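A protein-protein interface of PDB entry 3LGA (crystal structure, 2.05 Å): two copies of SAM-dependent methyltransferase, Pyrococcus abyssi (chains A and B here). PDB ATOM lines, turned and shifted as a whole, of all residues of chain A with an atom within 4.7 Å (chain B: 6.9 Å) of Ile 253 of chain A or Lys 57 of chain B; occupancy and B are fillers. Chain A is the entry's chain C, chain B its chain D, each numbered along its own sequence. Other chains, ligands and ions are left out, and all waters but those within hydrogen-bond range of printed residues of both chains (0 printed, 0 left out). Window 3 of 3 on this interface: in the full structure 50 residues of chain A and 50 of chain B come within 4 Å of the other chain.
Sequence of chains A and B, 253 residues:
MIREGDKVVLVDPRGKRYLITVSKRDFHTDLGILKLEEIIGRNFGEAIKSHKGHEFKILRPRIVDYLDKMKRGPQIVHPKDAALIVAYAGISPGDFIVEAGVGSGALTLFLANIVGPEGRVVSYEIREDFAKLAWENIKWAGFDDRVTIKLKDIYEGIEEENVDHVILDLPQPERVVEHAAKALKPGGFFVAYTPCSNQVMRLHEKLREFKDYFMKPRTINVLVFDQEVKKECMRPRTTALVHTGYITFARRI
No position is printed for both chains. Of the 4 pairs that touch across the chains among the printed residues, none has its exchanged pair printed and touching as well.
Among the printed residues, pairs that only touch across the chains: Pro 186 of chain A with Leu 59 of chain B, Pro 186 of chain A with Gly 45 of chain B, Pro 186 of chain A with Phe 44 of chain B and Ile 253 of chain A with Lys 57 of chain B.
O of Tyr 213 of chain A lies within hydrogen-bond range of N of Ile 253 of chain A, at 2.9 Å. The backbone carbonyl oxygen (O) of Ile 58 of chain B sits at hydrogen-bond distance from the backbone NH (N) of Gly 45 of chain B (2.8 Å). The backbone carbonyl oxygen (O) of Val 9 of chain B lies within hydrogen-bond range of the backbone NH (N) of Leu 59 of chain B, at 2.8 Å. The side-chain amino group of Lys 57 of chain B lies within salt-bridge range of the side-chain carboxylate of Glu 55 of chain B (3.7 Å). The backbone NH (N) of Val 11 of chain B is in hydrogen-bond range of the backbone carbonyl oxygen (O) of Lys 57 of chain B (2.8 Å).
Ile 253 of chain A touches just one residue of chain B: Lys 57 (3.96 Å). Leu 10 of chain B touches none of the printed residues of chain A. Printed residues of chain A within 4 Å of Phe 44 of chain B: Pro 186. Of chain A, only Ile 253 comes within 4 Å of Lys 57 of chain B. Printed residues of chain A within 4 Å of Leu 59 of chain B: Pro 186 (3.8 Å). The nearest printed residue of chain A that does not touch Lys 57 of chain B is Asp 212 of chain A (5.9 Å). The nearest printed residue of chain B that does not touch Pro 186 of chain A is Ile 58 of chain B (5.0 Å).
Of the 8 printed residues of chain A, 2 touch a printed residue of chain B. Hydrophobic or aromatic side chains of chain A within 4 Å of the printed part of chain B: Pro 186. Of the 16 printed residues of chain B, 4 touch a printed residue of chain A. Hydrophobic or aromatic side chains of chain B that line the printed part of chain A: Leu 59. Along chain B the printed residues that touch a printed residue of chain A span positions 44 to 59. Among the printed residues, 4 pairs touch across the chains. Among the printed residues, no Asp or Glu carboxylate lies within 4 Å of a Lys or Arg side-chain nitrogen of the other chain.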
ATOM      1  N   PRO A 186      28.888 -26.091 -10.519  1.00  0.00           N
ATOM      2  CA  PRO A 186      28.047 -24.917 -10.312  1.00  0.00           C
ATOM      3  C   PRO A 186      28.209 -24.423  -8.869  1.00  0.00           C
ATOM      4  O   PRO A 186      28.047 -25.193  -7.924  1.00  0.00           O
ATOM      5  CB  PRO A 186      26.616 -25.439 -10.519  1.00  0.00           C
ATOM      6  CG  PRO A 186      26.757 -26.765 -11.173  1.00  0.00           C
ATOM      7  CD  PRO A 186      28.143 -27.254 -11.049  1.00  0.00           C
ATOM      8  N   ASP A 212      29.951 -15.121 -18.872  1.00  0.00           N
ATOM      9  CA  ASP A 212      28.796 -16.003 -18.902  1.00  0.00           C
ATOM     10  C   ASP A 212      29.052 -17.310 -18.120  1.00  0.00           C
ATOM     11  O   ASP A 212      28.219 -18.230 -18.112  1.00  0.00           O
ATOM     12  CB  ASP A 212      28.446 -16.367 -20.356  1.00  0.00           C
ATOM     13  CG  ASP A 212      27.778 -15.213 -21.144  1.00  0.00           C
ATOM     14  OD1 ASP A 212      27.573 -14.085 -20.608  1.00  0.00           O
ATOM     15  OD2 ASP A 212      27.457 -15.470 -22.333  1.00  0.00           O
ATOM     16  N   TYR A 213      30.221 -17.413 -17.509  1.00  0.00           N
ATOM     17  CA  TYR A 213      30.597 -18.621 -16.806  1.00  0.00           C
ATOM     18  C   TYR A 213      30.788 -18.354 -15.322  1.00  0.00           C
ATOM     19  O   TYR A 213      30.803 -19.278 -14.525  1.00  0.00           O
ATOM     20  CB  TYR A 213      31.888 -19.179 -17.391  1.00  0.00           C
ATOM     21  CG  TYR A 213      31.774 -19.637 -18.833  1.00  0.00           C
ATOM     22  CD1 TYR A 213      31.731 -20.989 -19.139  1.00  0.00           C
ATOM     23  CD2 TYR A 213      31.721 -18.706 -19.890  1.00  0.00           C
ATOM     24  CE1 TYR A 213      31.641 -21.416 -20.452  1.00  0.00           C
ATOM     25  CE2 TYR A 213      31.614 -19.122 -21.220  1.00  0.00           C
ATOM     26  CZ  TYR A 213      31.579 -20.481 -21.487  1.00  0.00           C
ATOM     27  OH  TYR A 213      31.471 -20.923 -22.790  1.00  0.00           O
ATOM     28  N   PHE A 214      30.947 -17.092 -14.952  1.00  0.00           N
ATOM     29  CA  PHE A 214      31.240 -16.751 -13.558  1.00  0.00           C
ATOM     30  C   PHE A 214      30.357 -15.602 -13.118  1.00  0.00           C
ATOM     31  O   PHE A 214      29.920 -14.803 -13.951  1.00  0.00           O
ATOM     32  CB  PHE A 214      32.718 -16.387 -13.387  1.00  0.00           C
ATOM     33  CG  PHE A 214      33.680 -17.543 -13.582  1.00  0.00           C
ATOM     34  CD1 PHE A 214      34.297 -17.751 -14.798  1.00  0.00           C
ATOM     35  CD2 PHE A 214      33.974 -18.397 -12.534  1.00  0.00           C
ATOM     36  CE1 PHE A 214      35.192 -18.799 -14.986  1.00  0.00           C
ATOM     37  CE2 PHE A 214      34.850 -19.452 -12.692  1.00  0.00           C
ATOM     38  CZ  PHE A 214      35.483 -19.653 -13.940  1.00  0.00           C
ATOM     39  N   MET A 215      30.076 -15.504 -11.823  1.00  0.00           N
ATOM     40  CA  MET A 215      29.495 -14.276 -11.296  1.00  0.00           C
ATOM     41  C   MET A 215      30.551 -13.161 -11.276  1.00  0.00           C
ATOM     42  O   MET A 215      31.724 -13.386 -11.591  1.00  0.00           O
ATOM     43  CB  MET A 215      28.894 -14.514  -9.916  1.00  0.00           C
ATOM     44  CG  MET A 215      27.777 -15.531  -9.938  1.00  0.00           C
ATOM     45  SD  MET A 215      27.258 -16.107  -8.298  1.00  0.00           S
ATOM     46  CE  MET A 215      26.485 -14.630  -7.658  1.00  0.00           C
ATOM     47  N   ARG A 251      32.788 -16.804  -8.679  1.00  0.00           N
ATOM     48  CA  ARG A 251      31.978 -17.977  -8.452  1.00  0.00           C
ATOM     49  C   ARG A 251      31.411 -18.510  -9.766  1.00  0.00           C
ATOM     50  O   ARG A 251      30.785 -17.775 -10.497  1.00  0.00           O
ATOM     51  CB  ARG A 251      30.821 -17.767  -7.447  1.00  0.00           C
ATOM     52  CG  ARG A 251      30.743 -19.041  -6.631  1.00  0.00           C
ATOM     53  CD  ARG A 251      29.456 -19.724  -6.126  1.00  0.00           C
ATOM     54  NE  ARG A 251      28.743 -19.031  -5.131  1.00  0.00           N
ATOM     55  CZ  ARG A 251      27.857 -19.467  -4.213  1.00  0.00           C
ATOM     56  NH1 ARG A 251      27.553 -20.732  -3.874  1.00  0.00           N
ATOM     57  NH2 ARG A 251      27.286 -18.505  -3.533  1.00  0.00           N
ATOM     58  N   ARG A 252      31.570 -19.809  -9.990  1.00  0.00           N
ATOM     59  CA  ARG A 252      31.097 -20.466 -11.206  1.00  0.00           C
ATOM     60  C   ARG A 252      29.546 -20.567 -11.256  1.00  0.00           C
ATOM     61  O   ARG A 252      28.898 -20.972 -10.278  1.00  0.00           O
ATOM     62  CB  ARG A 252      31.742 -21.834 -11.325  1.00  0.00           C
ATOM     63  CG  ARG A 252      32.185 -22.234 -12.749  1.00  0.00           C
ATOM     64  CD  ARG A 252      31.228 -23.150 -13.423  1.00  0.00           C
ATOM     65  NE  ARG A 252      30.560 -22.390 -14.475  1.00  0.00           N
ATOM     66  CZ  ARG A 252      30.539 -22.691 -15.771  1.00  0.00           C
ATOM     67  NH1 ARG A 252      31.131 -23.781 -16.237  1.00  0.00           N
ATOM     68  NH2 ARG A 252      29.890 -21.896 -16.602  1.00  0.00           N
ATOM     69  N   ILE A 253      29.011 -20.177 -12.418  1.00  0.00           N
ATOM     70  CA  ILE A 253      27.584 -20.029 -12.819  1.00  0.00           C
ATOM     71  C   ILE A 253      26.530 -19.220 -12.080  1.00  0.00           C
ATOM     72  O   ILE A 253      26.627 -18.000 -12.222  1.00  0.00           O
ATOM     73  CB  ILE A 253      26.965 -21.171 -13.741  1.00  0.00           C
ATOM     74  CG1 ILE A 253      27.366 -22.613 -13.291  1.00  0.00           C
ATOM     75  CG2 ILE A 253      27.396 -20.885 -15.104  1.00  0.00           C
ATOM     76  CD1 ILE A 253      26.607 -23.857 -14.038  1.00  0.00           C
ATOM     77  OXT ILE A 253      25.528 -19.662 -11.490  1.00  0.00           O
ATOM     78  N   VAL B   8      17.865 -24.262  -1.397  1.00  0.00           N
ATOM     79  CA  VAL B   8      18.432 -23.957  -2.699  1.00  0.00           C
ATOM     80  C   VAL B   8      18.795 -22.473  -2.748  1.00  0.00           C
ATOM     81  O   VAL B   8      18.117 -21.655  -2.149  1.00  0.00           O
ATOM     82  CB  VAL B   8      17.367 -24.360  -3.778  1.00  0.00           C
ATOM     83  CG1 VAL B   8      17.146 -23.303  -4.849  1.00  0.00           C
ATOM     84  CG2 VAL B   8      17.653 -25.760  -4.323  1.00  0.00           C
ATOM     85  N   VAL B   9      19.872 -22.122  -3.441  1.00  0.00           N
ATOM     86  CA  VAL B   9      20.128 -20.721  -3.756  1.00  0.00           C
ATOM     87  C   VAL B   9      19.664 -20.435  -5.191  1.00  0.00           C
ATOM     88  O   VAL B   9      20.104 -21.106  -6.145  1.00  0.00           O
ATOM     89  CB  VAL B   9      21.630 -20.321  -3.601  1.00  0.00           C
ATOM     90  CG1 VAL B   9      21.871 -18.888  -4.131  1.00  0.00           C
ATOM     91  CG2 VAL B   9      22.070 -20.437  -2.143  1.00  0.00           C
ATOM     92  N   LEU B  10      18.788 -19.438  -5.338  1.00  0.00           N
ATOM     93  CA  LEU B  10      18.402 -18.952  -6.673  1.00  0.00           C
ATOM     94  C   LEU B  10      19.184 -17.723  -7.034  1.00  0.00           C
ATOM     95  O   LEU B  10      19.247 -16.787  -6.241  1.00  0.00           O
ATOM     96  CB  LEU B  10      16.891 -18.678  -6.765  1.00  0.00           C
ATOM     97  CG  LEU B  10      16.018 -19.915  -6.498  1.00  0.00           C
ATOM     98  CD1 LEU B  10      14.525 -19.524  -6.492  1.00  0.00           C
ATOM     99  CD2 LEU B  10      16.309 -21.035  -7.504  1.00  0.00           C
ATOM    100  N   VAL B  11      19.796 -17.731  -8.223  1.00  0.00           N
ATOM    101  CA  VAL B  11      20.598 -16.595  -8.689  1.00  0.00           C
ATOM    102  C   VAL B  11      19.874 -15.833  -9.833  1.00  0.00           C
ATOM    103  O   VAL B  11      19.551 -16.421 -10.877  1.00  0.00           O
ATOM    104  CB  VAL B  11      22.038 -17.005  -9.121  1.00  0.00           C
ATOM    105  CG1 VAL B  11      22.898 -15.775  -9.411  1.00  0.00           C
ATOM    106  CG2 VAL B  11      22.720 -17.862  -8.041  1.00  0.00           C
ATOM    107  N   ASP B  12      19.614 -14.545  -9.565  1.00  0.00           N
ATOM    108  CA  ASP B  12      19.127 -13.504 -10.501  1.00  0.00           C
ATOM    109  C   ASP B  12      19.981 -13.364 -11.730  1.00  0.00           C
ATOM    110  O   ASP B  12      21.183 -13.634 -11.660  1.00  0.00           O
ATOM    111  CB  ASP B  12      19.238 -12.114  -9.837  1.00  0.00           C
ATOM    112  CG  ASP B  12      17.912 -11.520  -9.520  1.00  0.00           C
ATOM    113  OD1 ASP B  12      16.914 -12.217  -9.778  1.00  0.00           O
ATOM    114  OD2 ASP B  12      17.848 -10.372  -9.023  1.00  0.00           O
ATOM    115  N   PRO B  13      19.381 -12.873 -12.850  1.00  0.00           N
ATOM    116  CA  PRO B  13      20.178 -12.365 -13.983  1.00  0.00           C
ATOM    117  C   PRO B  13      21.129 -11.230 -13.605  1.00  0.00           C
ATOM    118  O   PRO B  13      22.144 -11.048 -14.272  1.00  0.00           O
ATOM    119  CB  PRO B  13      19.111 -11.882 -14.975  1.00  0.00           C
ATOM    120  CG  PRO B  13      17.902 -12.716 -14.663  1.00  0.00           C
ATOM    121  CD  PRO B  13      17.931 -12.820 -13.149  1.00  0.00           C
ATOM    122  N   PHE B  44      21.146 -29.198  -9.491  1.00  0.00           N
ATOM    123  CA  PHE B  44      21.976 -27.987  -9.365  1.00  0.00           C
ATOM    124  C   PHE B  44      22.696 -27.652 -10.666  1.00  0.00           C
ATOM    125  O   PHE B  44      23.273 -28.517 -11.311  1.00  0.00           O
ATOM    126  CB  PHE B  44      22.962 -28.110  -8.198  1.00  0.00           C
ATOM    127  CG  PHE B  44      22.286 -28.297  -6.874  1.00  0.00           C
ATOM    128  CD1 PHE B  44      21.477 -27.295  -6.349  1.00  0.00           C
ATOM    129  CD2 PHE B  44      22.421 -29.485  -6.168  1.00  0.00           C
ATOM    130  CE1 PHE B  44      20.832 -27.456  -5.126  1.00  0.00           C
ATOM    131  CE2 PHE B  44      21.766 -29.665  -4.940  1.00  0.00           C
ATOM    132  CZ  PHE B  44      20.979 -28.636  -4.414  1.00  0.00           C
ATOM    133  N   GLY B  45      22.643 -26.388 -11.047  1.00  0.00           N
ATOM    134  CA  GLY B  45      23.192 -25.952 -12.316  1.00  0.00           C
ATOM    135  C   GLY B  45      22.089 -25.574 -13.292  1.00  0.00           C
ATOM    136  O   GLY B  45      22.304 -24.730 -14.175  1.00  0.00           O
ATOM    137  N   GLU B  46      20.906 -26.172 -13.124  1.00  0.00           N
ATOM    138  CA  GLU B  46      19.757 -25.862 -13.980  1.00  0.00           C
ATOM    139  C   GLU B  46      19.115 -24.551 -13.559  1.00  0.00           C
ATOM    140  O   GLU B  46      19.667 -23.832 -12.713  1.00  0.00           O
ATOM    141  CB  GLU B  46      18.746 -27.012 -13.994  1.00  0.00           C
ATOM    142  CG  GLU B  46      19.289 -28.278 -14.657  1.00  0.00           C
ATOM    143  CD  GLU B  46      18.401 -29.512 -14.465  1.00  0.00           C
ATOM    144  OE1 GLU B  46      17.176 -29.368 -14.219  1.00  0.00           O
ATOM    145  OE2 GLU B  46      18.941 -30.640 -14.576  1.00  0.00           O
ATOM    146  N   ALA B  47      17.974 -24.223 -14.168  1.00  0.00           N
ATOM    147  CA  ALA B  47      17.308 -22.936 -13.936  1.00  0.00           C
ATOM    148  C   ALA B  47      15.776 -23.025 -13.949  1.00  0.00           C
ATOM    149  O   ALA B  47      15.193 -23.965 -14.488  1.00  0.00           O
ATOM    150  CB  ALA B  47      17.794 -21.891 -14.935  1.00  0.00           C
ATOM    151  N   ILE B  48      15.153 -22.044 -13.308  1.00  0.00           N
ATOM    152  CA  ILE B  48      13.717 -21.805 -13.355  1.00  0.00           C
ATOM    153  C   ILE B  48      13.554 -20.413 -13.980  1.00  0.00           C
ATOM    154  O   ILE B  48      14.489 -19.600 -13.945  1.00  0.00           O
ATOM    155  CB  ILE B  48      13.089 -21.850 -11.924  1.00  0.00           C
ATOM    156  CG1 ILE B  48      13.225 -23.237 -11.314  1.00  0.00           C
ATOM    157  CG2 ILE B  48      11.613 -21.491 -11.923  1.00  0.00           C
ATOM    158  CD1 ILE B  48      12.773 -24.363 -12.212  1.00  0.00           C
ATOM    159  N   GLU B  55      15.277 -15.559 -15.890  1.00  0.00           N
ATOM    160  CA  GLU B  55      15.890 -16.818 -15.462  1.00  0.00           C
ATOM    161  C   GLU B  55      16.577 -16.763 -14.083  1.00  0.00           C
ATOM    162  O   GLU B  55      17.398 -15.881 -13.806  1.00  0.00           O
ATOM    163  CB  GLU B  55      16.891 -17.289 -16.507  1.00  0.00           C
ATOM    164  CG  GLU B  55      17.232 -18.746 -16.388  1.00  0.00           C
ATOM    165  CD  GLU B  55      18.081 -19.228 -17.539  1.00  0.00           C
ATOM    166  OE1 GLU B  55      19.273 -18.826 -17.612  1.00  0.00           O
ATOM    167  OE2 GLU B  55      17.549 -20.006 -18.372  1.00  0.00           O
ATOM    168  N   PHE B  56      16.230 -17.729 -13.238  1.00  0.00           N
ATOM    169  CA  PHE B  56      16.850 -17.882 -11.921  1.00  0.00           C
ATOM    170  C   PHE B  56      17.606 -19.209 -11.892  1.00  0.00           C
ATOM    171  O   PHE B  56      16.999 -20.280 -11.992  1.00  0.00           O
ATOM    172  CB  PHE B  56      15.805 -17.819 -10.800  1.00  0.00           C
ATOM    173  CG  PHE B  56      15.291 -16.424 -10.512  1.00  0.00           C
ATOM    174  CD1 PHE B  56      15.647 -15.770  -9.336  1.00  0.00           C
ATOM    175  CD2 PHE B  56      14.435 -15.771 -11.412  1.00  0.00           C
ATOM    176  CE1 PHE B  56      15.170 -14.498  -9.046  1.00  0.00           C
ATOM    177  CE2 PHE B  56      13.961 -14.491 -11.145  1.00  0.00           C
ATOM    178  CZ  PHE B  56      14.328 -13.847  -9.955  1.00  0.00           C
ATOM    179  N   LYS B  57      18.929 -19.129 -11.761  1.00  0.00           N
ATOM    180  CA  LYS B  57      19.784 -20.322 -11.716  1.00  0.00           C
ATOM    181  C   LYS B  57      19.804 -20.981 -10.319  1.00  0.00           C
ATOM    182  O   LYS B  57      19.750 -20.286  -9.307  1.00  0.00           O
ATOM    183  CB  LYS B  57      21.199 -19.960 -12.150  1.00  0.00           C
ATOM    184  CG  LYS B  57      21.283 -19.369 -13.552  1.00  0.00           C
ATOM    185  CD  LYS B  57      22.462 -18.402 -13.658  1.00  0.00           C
ATOM    186  CE  LYS B  57      22.492 -17.683 -15.015  1.00  0.00           C
ATOM    187  NZ  LYS B  57      22.648 -18.662 -16.133  1.00  0.00           N
ATOM    188  N   ILE B  58      19.912 -22.309 -10.285  1.00  0.00           N
ATOM    189  CA  ILE B  58      19.804 -23.097  -9.059  1.00  0.00           C
ATOM    190  C   ILE B  58      21.174 -23.613  -8.567  1.00  0.00           C
ATOM    191  O   ILE B  58      21.846 -24.368  -9.283  1.00  0.00           O
ATOM    192  CB  ILE B  58      18.844 -24.307  -9.261  1.00  0.00           C
ATOM    193  CG1 ILE B  58      17.488 -23.844  -9.842  1.00  0.00           C
ATOM    194  CG2 ILE B  58      18.670 -25.084  -7.954  1.00  0.00           C
ATOM    195  CD1 ILE B  58      16.667 -25.014 -10.477  1.00  0.00           C
ATOM    196  N   LEU B  59      21.583 -23.196  -7.359  1.00  0.00           N
ATOM    197  CA  LEU B  59      22.868 -23.636  -6.749  1.00  0.00           C
ATOM    198  C   LEU B  59      22.609 -24.327  -5.417  1.00  0.00           C
ATOM    199  O   LEU B  59      21.612 -24.008  -4.736  1.00  0.00           O
ATOM    200  CB  LEU B  59      23.801 -22.434  -6.482  1.00  0.00           C
ATOM    201  CG  LEU B  59      24.249 -21.596  -7.666  1.00  0.00           C
ATOM    202  CD1 LEU B  59      25.216 -20.498  -7.234  1.00  0.00           C
ATOM    203  CD2 LEU B  59      24.884 -22.531  -8.712  1.00  0.00           C
